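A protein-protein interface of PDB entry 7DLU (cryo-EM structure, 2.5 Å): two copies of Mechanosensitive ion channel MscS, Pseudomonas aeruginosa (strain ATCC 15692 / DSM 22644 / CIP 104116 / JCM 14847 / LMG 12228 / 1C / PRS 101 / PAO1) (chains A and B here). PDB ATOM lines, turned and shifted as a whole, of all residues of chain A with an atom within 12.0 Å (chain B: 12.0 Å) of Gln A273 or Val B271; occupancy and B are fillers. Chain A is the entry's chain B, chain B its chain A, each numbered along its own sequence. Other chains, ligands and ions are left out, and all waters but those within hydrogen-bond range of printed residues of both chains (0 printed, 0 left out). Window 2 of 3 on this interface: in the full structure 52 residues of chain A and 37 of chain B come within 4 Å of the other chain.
Along chain B the printed residues that touch a printed residue of chain A span positions 267 to 271.
Hydrophobic or aromatic side chains of chain A that line the printed part of chain B: Val A269 and Val A272.
Among the printed residues, no Asp or Glu carboxylate lies within 4 Å of a Lys or Arg side-chain nitrogen of the other chain.
Val A271 touches just one residue of chain B: Val B269.
Val A272 touches three residues of chain B.
Of chain A, only Val A269, Lys A270, Val A271 and Val A272 come within 4 Å of Val B269.
Of chain A, only Val A272 comes within 4 Å of Lys B270.
No residue of chain A comes within 4 Å of Gln B273.
Printed residues of chain B within 4 Å of Lys A270: Arg B267, Val B268 and Val B269.
Printed residues of chain B within 4 Å of Val A269: Arg B267 (3.4 Å) and Val B269 (3.8 Å).
Of the printed residues of chain B, Val A268 touches Arg B267 (2.8 Å).
The nearest printed residue of chain B that does not touch Val A268 is Val B268 (5.4 Å).
Lys A270 touches Val B268, but with the chains exchanged Val A268 does not touch Lys B270 (10.7 Å).
Lys A270 touches Val B269, but with the chains exchanged Val A269 does not touch Lys B270 (7.1 Å).
Val A271 touches Val B269, but with the chains exchanged Val A269 does not touch Val B271 (7.2 Å).
Val A272 touches Val B269, but with the chains exchanged Val A269 does not touch Val B272 (11.4 Å).
The backbone NH (N) of Arg B267 sits at hydrogen-bond distance from the backbone carbonyl oxygen (O) of Val A268, 2.8 Å away.
The backbone carbonyl oxygen (O) of Arg B267 lies within hydrogen-bond range of the backbone NH (N) of Lys A270.
N of Val B269 is in hydrogen-bond range of O of Lys A270 (3.1 Å).
The backbone carbonyl oxygen (O) of Val B269 is in hydrogen-bond range of the backbone NH (N) of Val A272, at 3.1 Å.
The backbone NH (N) of Val B271 lies within hydrogen-bond range of the backbone carbonyl oxygen (O) of Val A272, 3.3 Å away.
Val A269 touches Arg B267 (CA to O, 3.4 Å).
Val A269 touches Val B269 (CG1 to CG2, 3.8 Å).
CA of Val B268 touches O of Lys A270, 3.6 Å away.
CA of Val A271 touches O of Val B269 (3.5 Å).
Val A272 touches Lys B270 (O to CA, 3.3 Å).
Gln A273 touches Val B271.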
ATOM      1  N   VAL A 268      21.334   6.737 -23.988  1.00  0.00           N
ATOM      2  CA  VAL A 268      20.704   7.467 -25.083  1.00  0.00           C
ATOM      3  C   VAL A 268      21.140   8.919 -24.981  1.00  0.00           C
ATOM      4  O   VAL A 268      20.924   9.567 -23.950  1.00  0.00           O
ATOM      5  CB  VAL A 268      19.173   7.345 -25.052  1.00  0.00           C
ATOM      6  CG1 VAL A 268      18.564   8.043 -26.251  1.00  0.00           C
ATOM      7  CG2 VAL A 268      18.764   5.892 -25.027  1.00  0.00           C
ATOM      8  N   VAL A 269      21.753   9.430 -26.045  1.00  0.00           N
ATOM      9  CA  VAL A 269      22.377  10.747 -26.039  1.00  0.00           C
ATOM     10  C   VAL A 269      21.765  11.580 -27.155  1.00  0.00           C
ATOM     11  O   VAL A 269      21.804  11.182 -28.325  1.00  0.00           O
ATOM     12  CB  VAL A 269      23.902  10.660 -26.207  1.00  0.00           C
ATOM     13  CG1 VAL A 269      24.483  12.029 -26.483  1.00  0.00           C
ATOM     14  CG2 VAL A 269      24.530  10.054 -24.970  1.00  0.00           C
ATOM     15  N   LYS A 270      21.207  12.730 -26.796  1.00  0.00           N
ATOM     16  CA  LYS A 270      20.688  13.693 -27.758  1.00  0.00           C
ATOM     17  C   LYS A 270      21.727  14.787 -27.954  1.00  0.00           C
ATOM     18  O   LYS A 270      22.054  15.514 -27.011  1.00  0.00           O
ATOM     19  CB  LYS A 270      19.364  14.285 -27.279  1.00  0.00           C
ATOM     20  CG  LYS A 270      18.845  15.409 -28.147  1.00  0.00           C
ATOM     21  CD  LYS A 270      17.765  16.188 -27.430  1.00  0.00           C
ATOM     22  CE  LYS A 270      17.467  17.494 -28.135  1.00  0.00           C
ATOM     23  NZ  LYS A 270      16.590  18.365 -27.307  1.00  0.00           N
ATOM     24  N   VAL A 271      22.246  14.901 -29.171  1.00  0.00           N
ATOM     25  CA  VAL A 271      23.345  15.810 -29.467  1.00  0.00           C
ATOM     26  C   VAL A 271      22.780  17.118 -30.003  1.00  0.00           C
ATOM     27  O   VAL A 271      22.085  17.132 -31.024  1.00  0.00           O
ATOM     28  CB  VAL A 271      24.327  15.186 -30.469  1.00  0.00           C
ATOM     29  CG1 VAL A 271      25.345  16.217 -30.914  1.00  0.00           C
ATOM     30  CG2 VAL A 271      25.016  13.984 -29.854  1.00  0.00           C
ATOM     31  N   VAL A 272      23.080  18.216 -29.318  1.00  0.00           N
ATOM     32  CA  VAL A 272      22.759  19.559 -29.784  1.00  0.00           C
ATOM     33  C   VAL A 272      24.066  20.236 -30.171  1.00  0.00           C
ATOM     34  O   VAL A 272      25.002  20.308 -29.366  1.00  0.00           O
ATOM     35  CB  VAL A 272      21.994  20.365 -28.724  1.00  0.00           C
ATOM     36  CG1 VAL A 272      22.602  20.161 -27.347  1.00  0.00           C
ATOM     37  CG2 VAL A 272      21.987  21.836 -29.089  1.00  0.00           C
ATOM     38  N   GLN A 273      24.137  20.717 -31.407  1.00  0.00           N
ATOM     39  CA  GLN A 273      25.368  21.299 -31.927  1.00  0.00           C
ATOM     40  C   GLN A 273      25.212  22.794 -32.176  1.00  0.00           C
ATOM     41  O   GLN A 273      25.787  23.614 -31.461  1.00  0.00           O
ATOM     42  CB  GLN A 273      25.785  20.591 -33.217  1.00  0.00           C
ATOM     43  CG  GLN A 273      27.262  20.259 -33.295  1.00  0.00           C
ATOM     44  CD  GLN A 273      27.522  18.927 -33.969  1.00  0.00           C
ATOM     45  OE1 GLN A 273      26.754  18.493 -34.828  1.00  0.00           O
ATOM     46  NE2 GLN A 273      28.608  18.270 -33.583  1.00  0.00           N
ATOM     47  N   ARG B 267      20.625  11.377 -21.771  1.00  0.00           N
ATOM     48  CA  ARG B 267      21.621  12.423 -21.578  1.00  0.00           C
ATOM     49  C   ARG B 267      21.519  13.411 -22.729  1.00  0.00           C
ATOM     50  O   ARG B 267      21.234  13.031 -23.866  1.00  0.00           O
ATOM     51  CB  ARG B 267      23.040  11.853 -21.508  1.00  0.00           C
ATOM     52  CG  ARG B 267      23.629  11.811 -20.113  1.00  0.00           C
ATOM     53  CD  ARG B 267      24.344  10.501 -19.881  1.00  0.00           C
ATOM     54  NE  ARG B 267      24.587  10.241 -18.468  1.00  0.00           N
ATOM     55  CZ  ARG B 267      23.665   9.811 -17.615  1.00  0.00           C
ATOM     56  NH1 ARG B 267      22.425   9.595 -18.022  1.00  0.00           N
ATOM     57  NH2 ARG B 267      23.983   9.599 -16.348  1.00  0.00           N
ATOM     58  N   VAL B 268      21.752  14.685 -22.424  1.00  0.00           N
ATOM     59  CA  VAL B 268      21.776  15.748 -23.422  1.00  0.00           C
ATOM     60  C   VAL B 268      23.180  16.330 -23.443  1.00  0.00           C
ATOM     61  O   VAL B 268      23.679  16.797 -22.414  1.00  0.00           O
ATOM     62  CB  VAL B 268      20.731  16.836 -23.133  1.00  0.00           C
ATOM     63  CG1 VAL B 268      20.731  17.874 -24.238  1.00  0.00           C
ATOM     64  CG2 VAL B 268      19.359  16.220 -22.992  1.00  0.00           C
ATOM     65  N   VAL B 269      23.816  16.300 -24.611  1.00  0.00           N
ATOM     66  CA  VAL B 269      25.220  16.663 -24.754  1.00  0.00           C
ATOM     67  C   VAL B 269      25.332  17.780 -25.780  1.00  0.00           C
ATOM     68  O   VAL B 269      24.896  17.621 -26.926  1.00  0.00           O
ATOM     69  CB  VAL B 269      26.083  15.461 -25.171  1.00  0.00           C
ATOM     70  CG1 VAL B 269      27.463  15.920 -25.585  1.00  0.00           C
ATOM     71  CG2 VAL B 269      26.171  14.464 -24.035  1.00  0.00           C
ATOM     72  N   LYS B 270      25.917  18.901 -25.372  1.00  0.00           N
ATOM     73  CA  LYS B 270      26.207  20.013 -26.267  1.00  0.00           C
ATOM     74  C   LYS B 270      27.673  19.938 -26.670  1.00  0.00           C
ATOM     75  O   LYS B 270      28.560  20.051 -25.820  1.00  0.00           O
ATOM     76  CB  LYS B 270      25.900  21.350 -25.596  1.00  0.00           C
ATOM     77  CG  LYS B 270      26.327  22.555 -26.403  1.00  0.00           C
ATOM     78  CD  LYS B 270      26.346  23.798 -25.543  1.00  0.00           C
ATOM     79  CE  LYS B 270      27.074  24.934 -26.232  1.00  0.00           C
ATOM     80  NZ  LYS B 270      27.306  26.070 -25.301  1.00  0.00           N
ATOM     81  N   VAL B 271      27.923  19.744 -27.960  1.00  0.00           N
ATOM     82  CA  VAL B 271      29.271  19.516 -28.465  1.00  0.00           C
ATOM     83  C   VAL B 271      29.854  20.838 -28.944  1.00  0.00           C
ATOM     84  O   VAL B 271      29.296  21.487 -29.835  1.00  0.00           O
ATOM     85  CB  VAL B 271      29.272  18.477 -29.594  1.00  0.00           C
ATOM     86  CG1 VAL B 271      30.641  18.403 -30.238  1.00  0.00           C
ATOM     87  CG2 VAL B 271      28.857  17.118 -29.062  1.00  0.00           C
ATOM     88  N   VAL B 272      30.977  21.235 -28.356  1.00  0.00           N
ATOM     89  CA  VAL B 272      31.749  22.386 -28.808  1.00  0.00           C
ATOM     90  C   VAL B 272      33.036  21.861 -29.430  1.00  0.00           C
ATOM     91  O   VAL B 272      33.782  21.107 -28.794  1.00  0.00           O
ATOM     92  CB  VAL B 272      32.033  23.370 -27.663  1.00  0.00           C
ATOM     93  CG1 VAL B 272      32.437  22.630 -26.400  1.00  0.00           C
ATOM     94  CG2 VAL B 272      33.112  24.353 -28.072  1.00  0.00           C
ATOM     95  N   GLN B 273      33.288  22.245 -30.676  1.00  0.00           N
ATOM     96  CA  GLN B 273      34.435  21.732 -31.413  1.00  0.00           C
ATOM     97  C   GLN B 273      35.457  22.830 -31.683  1.00  0.00           C
ATOM     98  O   GLN B 273      36.541  22.838 -31.101  1.00  0.00           O
ATOM     99  CB  GLN B 273      33.980  21.101 -32.729  1.00  0.00           C
ATOM    100  CG  GLN B 273      34.637  19.769 -33.040  1.00  0.00           C
ATOM    101  CD  GLN B 273      33.685  18.795 -33.702  1.00  0.00           C
ATOM    102  OE1 GLN B 273      32.758  19.197 -34.406  1.00  0.00           O
ATOM    103  NE2 GLN B 273      33.908  17.506 -33.480  1.00  0.00           N
